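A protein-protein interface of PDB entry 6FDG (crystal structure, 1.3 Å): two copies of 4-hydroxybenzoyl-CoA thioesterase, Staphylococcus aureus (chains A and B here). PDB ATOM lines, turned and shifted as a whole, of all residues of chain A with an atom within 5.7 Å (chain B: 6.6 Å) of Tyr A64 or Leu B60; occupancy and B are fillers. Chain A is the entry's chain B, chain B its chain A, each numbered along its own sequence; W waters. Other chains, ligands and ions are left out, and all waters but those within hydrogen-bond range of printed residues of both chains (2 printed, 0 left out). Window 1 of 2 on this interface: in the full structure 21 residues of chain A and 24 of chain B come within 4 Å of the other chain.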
ATOM      1  N   HIS A  23      -7.762  28.941  -3.424  1.00  0.00           N
ATOM      2  CA  HIS A  23      -8.980  29.040  -2.663  1.00  0.00           C
ATOM      3  C   HIS A  23      -9.017  30.259  -1.782  1.00  0.00           C
ATOM      4  O   HIS A  23     -10.080  30.861  -1.543  1.00  0.00           O
ATOM      5  CB  HIS A  23      -9.231  27.799  -1.819  1.00  0.00           C
ATOM      6  CG  HIS A  23      -8.314  27.594  -0.670  1.00  0.00           C
ATOM      7  ND1 HIS A  23      -7.039  27.108  -0.794  1.00  0.00           N
ATOM      8  CD2 HIS A  23      -8.518  27.798   0.658  1.00  0.00           C
ATOM      9  CE1 HIS A  23      -6.495  27.033   0.467  1.00  0.00           C
ATOM     10  NE2 HIS A  23      -7.393  27.456   1.349  1.00  0.00           N
ATOM     11  N   GLY A  24      -7.813  30.713  -1.295  1.00  0.00           N
ATOM     12  CA  GLY A  24      -7.758  31.902  -0.465  1.00  0.00           C
ATOM     13  C   GLY A  24      -8.013  33.151  -1.176  1.00  0.00           C
ATOM     14  O   GLY A  24      -8.287  34.185  -0.492  1.00  0.00           O
ATOM     15  N   TYR A  26     -10.610  33.861  -3.077  1.00  0.00           N
ATOM     16  CA  TYR A  26     -12.049  34.023  -3.256  1.00  0.00           C
ATOM     17  C   TYR A  26     -12.598  35.093  -2.322  1.00  0.00           C
ATOM     18  O   TYR A  26     -13.509  35.868  -2.753  1.00  0.00           O
ATOM     19  CB  TYR A  26     -12.828  32.749  -3.107  1.00  0.00           C
ATOM     20  CG  TYR A  26     -12.669  31.825  -4.322  1.00  0.00           C
ATOM     21  CD1 TYR A  26     -11.501  31.193  -4.695  1.00  0.00           C
ATOM     22  CD2 TYR A  26     -13.794  31.558  -5.156  1.00  0.00           C
ATOM     23  CE1 TYR A  26     -11.417  30.302  -5.765  1.00  0.00           C
ATOM     24  CE2 TYR A  26     -13.716  30.682  -6.198  1.00  0.00           C
ATOM     25  CZ  TYR A  26     -12.540  30.060  -6.497  1.00  0.00           C
ATOM     26  OH  TYR A  26     -12.559  29.109  -7.536  1.00  0.00           O
ATOM     27  N   LEU A  60     -16.561  34.275   7.354  1.00  0.00           N
ATOM     28  CA  LEU A  60     -16.343  33.967   5.918  1.00  0.00           C
ATOM     29  C   LEU A  60     -16.692  32.548   5.686  1.00  0.00           C
ATOM     30  O   LEU A  60     -16.168  31.634   6.436  1.00  0.00           O
ATOM     31  CB  LEU A  60     -14.954  34.269   5.539  1.00  0.00           C
ATOM     32  CG  LEU A  60     -14.469  33.796   4.110  1.00  0.00           C
ATOM     33  CD1 LEU A  60     -15.147  34.591   3.027  1.00  0.00           C
ATOM     34  CD2 LEU A  60     -12.987  33.932   4.024  1.00  0.00           C
ATOM     35  N   ASN A  61     -17.516  32.230   4.687  1.00  0.00           N
ATOM     36  CA  ASN A  61     -17.756  30.848   4.281  1.00  0.00           C
ATOM     37  C   ASN A  61     -17.644  30.778   2.787  1.00  0.00           C
ATOM     38  O   ASN A  61     -18.179  31.636   2.076  1.00  0.00           O
ATOM     39  CB  ASN A  61     -19.159  30.427   4.689  1.00  0.00           C
ATOM     40  CG  ASN A  61     -19.309  30.522   6.238  1.00  0.00           C
ATOM     41  OD1 ASN A  61     -18.787  29.657   6.961  1.00  0.00           O
ATOM     42  ND2 ASN A  61     -19.857  31.668   6.752  1.00  0.00           N
ATOM     43  N   VAL A  62     -16.962  29.759   2.278  1.00  0.00           N
ATOM     44  CA  VAL A  62     -16.802  29.522   0.829  1.00  0.00           C
ATOM     45  C   VAL A  62     -17.031  28.069   0.603  1.00  0.00           C
ATOM     46  O   VAL A  62     -16.340  27.231   1.247  1.00  0.00           O
ATOM     47  CB  VAL A  62     -15.471  30.019   0.222  1.00  0.00           C
ATOM     48  CG1 VAL A  62     -15.608  30.121  -1.237  1.00  0.00           C
ATOM     49  CG2 VAL A  62     -15.067  31.365   0.829  1.00  0.00           C
ATOM     50  N   ASN A  63     -17.884  27.692  -0.338  1.00  0.00           N
ATOM     51  CA  ASN A  63     -18.123  26.340  -0.815  1.00  0.00           C
ATOM     52  C   ASN A  63     -17.792  26.210  -2.222  1.00  0.00           C
ATOM     53  O   ASN A  63     -18.385  26.860  -3.108  1.00  0.00           O
ATOM     54  CB  ASN A  63     -19.553  25.863  -0.546  1.00  0.00           C
ATOM     55  CG  ASN A  63     -19.609  24.356  -0.752  1.00  0.00           C
ATOM     56  OD1 ASN A  63     -19.954  23.937  -1.770  1.00  0.00           O
ATOM     57  ND2 ASN A  63     -19.050  23.544   0.201  1.00  0.00           N
ATOM     58  N   TYR A  64     -16.744  25.431  -2.566  1.00  0.00           N
ATOM     59  CA  TYR A  64     -16.142  25.387  -3.903  1.00  0.00           C
ATOM     60  C   TYR A  64     -16.758  24.224  -4.709  1.00  0.00           C
ATOM     61  O   TYR A  64     -16.413  23.058  -4.414  1.00  0.00           O
ATOM     62  CB  TYR A  64     -14.614  25.234  -3.849  1.00  0.00           C
ATOM     63  CG  TYR A  64     -13.927  26.337  -3.027  1.00  0.00           C
ATOM     64  CD1 TYR A  64     -13.795  26.193  -1.638  1.00  0.00           C
ATOM     65  CD2 TYR A  64     -13.462  27.520  -3.564  1.00  0.00           C
ATOM     66  CE1 TYR A  64     -13.206  27.160  -0.861  1.00  0.00           C
ATOM     67  CE2 TYR A  64     -12.881  28.467  -2.790  1.00  0.00           C
ATOM     68  CZ  TYR A  64     -12.757  28.297  -1.475  1.00  0.00           C
ATOM     69  OH  TYR A  64     -12.172  29.266  -0.643  1.00  0.00           O
ATOM     70  N   LYS A  65     -17.665  24.452  -5.605  1.00  0.00           N
ATOM     71  CA  LYS A  65     -18.354  23.393  -6.366  1.00  0.00           C
ATOM     72  C   LYS A  65     -17.513  23.038  -7.546  1.00  0.00           C
ATOM     73  O   LYS A  65     -17.546  21.801  -7.896  1.00  0.00           O
ATOM     74  CB  LYS A  65     -19.687  23.870  -6.757  1.00  0.00           C
ATOM     75  CG  LYS A  65     -20.549  24.006  -5.446  1.00  0.00           C
ATOM     76  CD  LYS A  65     -21.772  24.745  -5.638  1.00  0.00           C
ATOM     77  CE  LYS A  65     -22.050  25.262  -4.210  1.00  0.00           C
ATOM     78  NZ  LYS A  65     -22.401  24.317  -3.141  1.00  0.00           N
ATOM     79  N   LYS A  66     -16.893  23.928  -8.283  1.00  0.00           N
ATOM     80  CA  LYS A  66     -16.066  23.646  -9.430  1.00  0.00           C
ATOM     81  C   LYS A  66     -14.857  24.529  -9.379  1.00  0.00           C
ATOM     82  O   LYS A  66     -14.963  25.676  -8.925  1.00  0.00           O
ATOM     83  CB  LYS A  66     -16.792  24.083 -10.777  1.00  0.00           C
ATOM     84  CG  LYS A  66     -18.121  23.355 -10.946  1.00  0.00           C
ATOM     85  CD  LYS A  66     -18.692  23.730 -12.291  1.00  0.00           C
ATOM     86  CE  LYS A  66     -19.990  23.029 -12.658  1.00  0.00           C
ATOM     87  NZ  LYS A  66     -19.833  21.543 -12.555  1.00  0.00           N
ATOM     88  N   ALA A 102     -20.145  27.746  -9.922  1.00  0.00           N
ATOM     89  CA  ALA A 102     -18.843  27.256  -9.478  1.00  0.00           C
ATOM     90  C   ALA A 102     -18.603  27.351  -7.941  1.00  0.00           C
ATOM     91  O   ALA A 102     -17.791  26.578  -7.427  1.00  0.00           O
ATOM     92  CB  ALA A 102     -17.758  27.948 -10.194  1.00  0.00           C
ATOM     93  N   THR A 103     -19.272  28.314  -7.304  1.00  0.00           N
ATOM     94  CA  THR A 103     -18.938  28.656  -5.908  1.00  0.00           C
ATOM     95  C   THR A 103     -20.115  29.296  -5.241  1.00  0.00           C
ATOM     96  O   THR A 103     -20.828  30.079  -5.887  1.00  0.00           O
ATOM     97  CB  THR A 103     -17.801  29.723  -5.909  1.00  0.00           C
ATOM     98  OG1 THR A 103     -16.890  29.565  -6.945  1.00  0.00           O
ATOM     99  CG2 THR A 103     -17.093  29.700  -4.515  1.00  0.00           C
ATOM    100  N   THR A 104     -20.352  28.996  -3.972  1.00  0.00           N
ATOM    101  CA  THR A 104     -21.286  29.739  -3.164  1.00  0.00           C
ATOM    102  C   THR A 104     -20.547  30.175  -1.923  1.00  0.00           C
ATOM    103  O   THR A 104     -19.452  29.681  -1.567  1.00  0.00           O
ATOM    104  CB  THR A 104     -22.505  28.949  -2.763  1.00  0.00           C
ATOM    105  OG1 THR A 104     -22.092  27.794  -2.036  1.00  0.00           O
ATOM    106  CG2 THR A 104     -23.239  28.556  -4.025  1.00  0.00           C
ATOM    107  N   GLY B  24      -8.849  37.851   4.149  1.00  0.00           N
ATOM    108  CA  GLY B  24      -8.567  36.833   3.118  1.00  0.00           C
ATOM    109  C   GLY B  24      -7.288  36.128   3.299  1.00  0.00           C
ATOM    110  O   GLY B  24      -7.111  35.089   2.597  1.00  0.00           O
ATOM    111  N   TYR B  26      -6.210  34.614   6.020  1.00  0.00           N
ATOM    112  CA  TYR B  26      -6.241  33.574   7.036  1.00  0.00           C
ATOM    113  C   TYR B  26      -6.264  32.200   6.416  1.00  0.00           C
ATOM    114  O   TYR B  26      -5.730  31.269   7.013  1.00  0.00           O
ATOM    115  CB  TYR B  26      -7.456  33.787   7.946  1.00  0.00           C
ATOM    116  CG  TYR B  26      -7.304  34.919   8.962  1.00  0.00           C
ATOM    117  CD1 TYR B  26      -7.229  36.273   8.647  1.00  0.00           C
ATOM    118  CD2 TYR B  26      -7.191  34.578  10.271  1.00  0.00           C
ATOM    119  CE1 TYR B  26      -7.145  37.267   9.584  1.00  0.00           C
ATOM    120  CE2 TYR B  26      -7.149  35.629  11.253  1.00  0.00           C
ATOM    121  CZ  TYR B  26      -7.120  36.898  10.858  1.00  0.00           C
ATOM    122  OH  TYR B  26      -7.092  37.903  11.878  1.00  0.00           O
ATOM    123  N   ALA B  27      -6.820  32.025   5.211  1.00  0.00           N
ATOM    124  CA  ALA B  27      -6.731  30.729   4.555  1.00  0.00           C
ATOM    125  C   ALA B  27      -5.297  30.293   4.370  1.00  0.00           C
ATOM    126  O   ALA B  27      -5.016  29.076   4.519  1.00  0.00           O
ATOM    127  CB  ALA B  27      -7.490  30.749   3.278  1.00  0.00           C
ATOM    128  N   PHE B  30      -4.132  28.930   7.658  1.00  0.00           N
ATOM    129  CA  PHE B  30      -4.689  27.570   7.882  1.00  0.00           C
ATOM    130  C   PHE B  30      -3.897  26.592   7.049  1.00  0.00           C
ATOM    131  O   PHE B  30      -3.658  25.461   7.538  1.00  0.00           O
ATOM    132  CB  PHE B  30      -6.139  27.495   7.530  1.00  0.00           C
ATOM    133  CG  PHE B  30      -7.088  28.233   8.450  1.00  0.00           C
ATOM    134  CD1 PHE B  30      -6.759  28.789   9.665  1.00  0.00           C
ATOM    135  CD2 PHE B  30      -8.442  28.265   8.082  1.00  0.00           C
ATOM    136  CE1 PHE B  30      -7.718  29.426  10.483  1.00  0.00           C
ATOM    137  CE2 PHE B  30      -9.405  28.838   8.894  1.00  0.00           C
ATOM    138  CZ  PHE B  30      -9.004  29.432  10.095  1.00  0.00           C
ATOM    139  N   VAL B  57      -8.713  22.339  -1.209  1.00  0.00           N
ATOM    140  CA  VAL B  57      -9.864  22.764  -0.291  1.00  0.00           C
ATOM    141  C   VAL B  57     -11.133  22.824  -0.996  1.00  0.00           C
ATOM    142  O   VAL B  57     -11.199  23.543  -2.032  1.00  0.00           O
ATOM    143  CB  VAL B  57      -9.465  24.082   0.356  1.00  0.00           C
ATOM    144  CG1 VAL B  57     -10.649  24.590   1.141  1.00  0.00           C
ATOM    145  CG2 VAL B  57      -8.292  23.897   1.240  1.00  0.00           C
ATOM    146  N   THR B  58     -12.194  22.234  -0.516  1.00  0.00           N
ATOM    147  CA  THR B  58     -13.507  22.247  -1.029  1.00  0.00           C
ATOM    148  C   THR B  58     -14.503  23.035  -0.216  1.00  0.00           C
ATOM    149  O   THR B  58     -15.605  23.379  -0.707  1.00  0.00           O
ATOM    150  CB  THR B  58     -14.033  20.804  -1.310  1.00  0.00           C
ATOM    151  OG1 THR B  58     -14.172  20.137  -0.052  1.00  0.00           O
ATOM    152  CG2 THR B  58     -13.136  20.160  -2.359  1.00  0.00           C
ATOM    153  N   ASP B  59     -14.142  23.422   1.025  1.00  0.00           N
ATOM    154  CA  ASP B  59     -15.018  24.260   1.865  1.00  0.00           C
ATOM    155  C   ASP B  59     -14.142  24.964   2.805  1.00  0.00           C
ATOM    156  O   ASP B  59     -13.213  24.361   3.424  1.00  0.00           O
ATOM    157  CB  ASP B  59     -16.022  23.454   2.677  1.00  0.00           C
ATOM    158  CG  ASP B  59     -17.066  24.247   3.275  1.00  0.00           C
ATOM    159  OD1 ASP B  59     -17.950  24.693   2.546  1.00  0.00           O
ATOM    160  OD2 ASP B  59     -17.009  24.466   4.471  1.00  0.00           O
ATOM    161  N   LEU B  60     -14.349  26.242   3.048  1.00  0.00           N
ATOM    162  CA  LEU B  60     -13.551  27.110   3.928  1.00  0.00           C
ATOM    163  C   LEU B  60     -14.510  27.820   4.872  1.00  0.00           C
ATOM    164  O   LEU B  60     -15.513  28.429   4.354  1.00  0.00           O
ATOM    165  CB  LEU B  60     -12.720  28.125   3.143  1.00  0.00           C
ATOM    166  CG  LEU B  60     -12.053  29.233   3.964  1.00  0.00           C
ATOM    167  CD1 LEU B  60     -10.916  28.662   4.838  1.00  0.00           C
ATOM    168  CD2 LEU B  60     -11.506  30.247   3.003  1.00  0.00           C
ATOM    169  N   ASN B  61     -14.247  27.860   6.172  1.00  0.00           N
ATOM    170  CA  ASN B  61     -14.991  28.673   7.129  1.00  0.00           C
ATOM    171  C   ASN B  61     -14.021  29.322   8.016  1.00  0.00           C
ATOM    172  O   ASN B  61     -13.073  28.729   8.509  1.00  0.00           O
ATOM    173  CB  ASN B  61     -15.896  27.764   7.939  1.00  0.00           C
ATOM    174  CG  ASN B  61     -16.795  26.908   7.016  1.00  0.00           C
ATOM    175  OD1 ASN B  61     -16.470  25.711   6.665  1.00  0.00           O
ATOM    176  ND2 ASN B  61     -17.858  27.473   6.534  1.00  0.00           N
ATOM    177  N   VAL B  62     -14.194  30.642   8.259  1.00  0.00           N
ATOM    178  CA  VAL B  62     -13.353  31.405   9.195  1.00  0.00           C
ATOM    179  C   VAL B  62     -14.273  32.271  10.054  1.00  0.00           C
ATOM    180  O   VAL B  62     -15.143  32.967   9.497  1.00  0.00           O
ATOM    181  CB  VAL B  62     -12.348  32.329   8.540  1.00  0.00           C
ATOM    182  CG1 VAL B  62     -11.310  32.817   9.511  1.00  0.00           C
ATOM    183  CG2 VAL B  62     -11.584  31.625   7.321  1.00  0.00           C
ATOM    184  N   TYR B  92      -9.433  24.584  13.196  1.00  0.00           N
ATOM    185  CA  TYR B  92      -8.358  25.436  13.654  1.00  0.00           C
ATOM    186  C   TYR B  92      -8.792  26.426  14.710  1.00  0.00           C
ATOM    187  O   TYR B  92      -9.948  26.905  14.739  1.00  0.00           O
ATOM    188  CB  TYR B  92      -7.841  26.347  12.521  1.00  0.00           C
ATOM    189  CG  TYR B  92      -7.536  25.553  11.245  1.00  0.00           C
ATOM    190  CD1 TYR B  92      -8.575  25.361  10.298  1.00  0.00           C
ATOM    191  CD2 TYR B  92      -6.293  25.096  10.958  1.00  0.00           C
ATOM    192  CE1 TYR B  92      -8.358  24.599   9.148  1.00  0.00           C
ATOM    193  CE2 TYR B  92      -6.052  24.359   9.763  1.00  0.00           C
ATOM    194  CZ  TYR B  92      -7.078  24.183   8.864  1.00  0.00           C
ATOM    195  OH  TYR B  92      -6.823  23.481   7.642  1.00  0.00           O
ATOM    196  N   SER B 106     -12.449  26.190   9.740  1.00  0.00           N
ATOM    197  CA  SER B 106     -12.362  24.842   9.265  1.00  0.00           C
ATOM    198  C   SER B 106     -12.106  24.815   7.789  1.00  0.00           C
ATOM    199  O   SER B 106     -12.400  25.780   7.046  1.00  0.00           O
ATOM    200  CB  SER B 106     -13.603  24.031   9.561  1.00  0.00           C
ATOM    201  OG  SER B 106     -14.756  24.566   8.969  1.00  0.00           O
ATOM    202  N   THR B 107     -11.520  23.739   7.296  1.00  0.00           N
ATOM    203  CA  THR B 107     -11.341  23.444   5.874  1.00  0.00           C
ATOM    204  C   THR B 107     -11.667  22.017   5.554  1.00  0.00           C
ATOM    205  O   THR B 107     -11.086  21.084   6.246  1.00  0.00           O
ATOM    206  CB  THR B 107      -9.947  23.706   5.369  1.00  0.00           C
ATOM    207  OG1 THR B 107      -9.006  22.897   6.143  1.00  0.00           O
ATOM    208  CG2 THR B 107      -9.525  25.190   5.437  1.00  0.00           C
ATOM    209  N   GLU B 108     -12.482  21.753   4.543  1.00  0.00           N
ATOM    210  CA  GLU B 108     -12.666  20.377   3.997  1.00  0.00           C
ATOM    211  C   GLU B 108     -11.716  20.229   2.874  1.00  0.00           C
ATOM    212  O   GLU B 108     -11.578  21.098   1.993  1.00  0.00           O
ATOM    213  CB  GLU B 108     -14.109  20.245   3.571  1.00  0.00           C
ATOM    214  CG  GLU B 108     -14.397  18.794   2.999  1.00  0.00           C
ATOM    215  CD  GLU B 108     -15.806  18.759   2.493  1.00  0.00           C
ATOM    216  OE1 GLU B 108     -16.102  19.558   1.583  1.00  0.00           O
ATOM    217  OE2 GLU B 108     -16.580  17.949   2.966  1.00  0.00           O
HETATM  218  O   HOH W   1      -6.327  26.671   3.777  1.00  0.00           O
HETATM  219  O   HOH W   2      -9.529  33.554   2.109  1.00  0.00           O
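Hydrophobic or aromatic side chains of chain B that line the printed part of chain A: Ala B27, Val B57 and Leu B60. Along chain B the printed residues that touch a printed residue of chain A span positions 24 to 62. Printed residues of chain A that touch a printed residue of chain B: His A23, Gly A24, Leu A60, Asn A61, Val A62, Asn A63 and Tyr A64. Among the printed residues, no Asp or Glu carboxylate lies within 4 Å of a Lys or Arg side-chain nitrogen of the other chain.
Water W1 bridges a ring nitrogen (NE2) of His A23 and the backbone carbonyl oxygen (O) of Ala B27. Water W2 bridges the backbone carbonyl oxygen (O) of Gly B24 and the backbone carbonyl oxygen (O) of Gly A24.
NE2 of His A23 touches CB of Ala B27, 3.8 Å away. CG2 of Val B57 touches NE2 of His A23, at 3.7 Å. Gly A24 touches Ala B27 (CA to CB, 3.9 Å). Leu B60 touches Leu A60. Leu A60 touches Asn B61. Asn A61 touches Leu B60 (CA to O, 3.3 Å). Asn A63 touches Thr B58. Tyr A64 touches Val B57 (CD1 to O, 3.7 Å). Tyr A64 touches Asp B59 (CD1 to N, 3.9 Å). Leu B60 touches Tyr A64 (CD2 to OH, 3.8 Å).
OG1 of Thr B58 lies within hydrogen-bond range of OE1 of Glu B108 (2.6 Å). OD1 of Asn B61 lies close to OD2 of Asp B59 (2.6 Å). The backbone NH of Glu B108 sits at hydrogen-bond distance from the backbone carbonyl oxygen of Asp B59 (2.9 Å). The side-chain hydroxyl (OH) of Tyr A64 is in hydrogen-bond range of the backbone carbonyl oxygen (O) of His A23, 2.8 Å away. OD1 of Asn A63 sits at hydrogen-bond distance from NZ of Lys A65 (2.8 Å). N of Asn A63 sits at hydrogen-bond distance from O of Thr A104, at 2.8 Å.
Printed residues of chain B within 4 Å of His A23: Ala B27 and Val B57. Of the printed residues of chain B, Asn A61 touches Leu B60 and Asn B61. Of the printed residues of chain B, Tyr A64 touches Val B57, Thr B58, Asp B59 and Leu B60. Thr A103 touches none of the printed residues of chain B. Printed residues of chain A within 4 Å of Gly B24: Gly A24. Printed residues of chain A within 4 Å of Ala B27: His A23 (3.8 Å) and Gly A24 (3.9 Å). Of the printed residues of chain A, Val B57 touches His A23 and Tyr A64. Of chain A, only Leu A60 (3.9 Å), Asn A61 (3.3 Å), Val A62 (2.9 Å) and Tyr A64 (3.8 Å) come within 4 Å of Leu B60. Ser B106 touches none of the printed residues of chain A. The nearest residue of chain A that does not touch Leu B60 is His A23 (4.5 Å).
The backbone NH (N) of Tyr A64 lies within hydrogen-bond range of the backbone carbonyl oxygen (O) of Thr B58 (3.0 Å). OD1 of Asp B59 lies within hydrogen-bond range of ND2 of Asn A63, 2.8 Å away. The backbone carbonyl oxygen of Leu B60 is in hydrogen-bond range of the backbone NH of Val A62. The side-chain amide oxygen (OD1) of Asn A61 is in hydrogen-bond range of the side-chain amide nitrogen (ND2) of Asn B61 (2.4 Å). N of Val B62 is in hydrogen-bond range of O of Leu A60. The backbone carbonyl oxygen (O) of Gly A24 lies close to the backbone carbonyl oxygen (O) of Gly B24 (3.4 Å). The backbone carbonyl oxygen (O) of Val A62 lies close to the side-chain carboxylate (OD1) of Asp B59, at 3.3 Å.
Gly A24 touches its own counterpart, Gly B24. Leu A60 touches its own counterpart, Leu B60. Leu A60 touches Asn B61, and with the chains exchanged Asn A61 touches Leu B60. Asn A61 touches its own counterpart, Asn B61. Of the 17 pairs that touch across the chains among the printed residues, 7 have their exchanged pair printed and touching as well.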
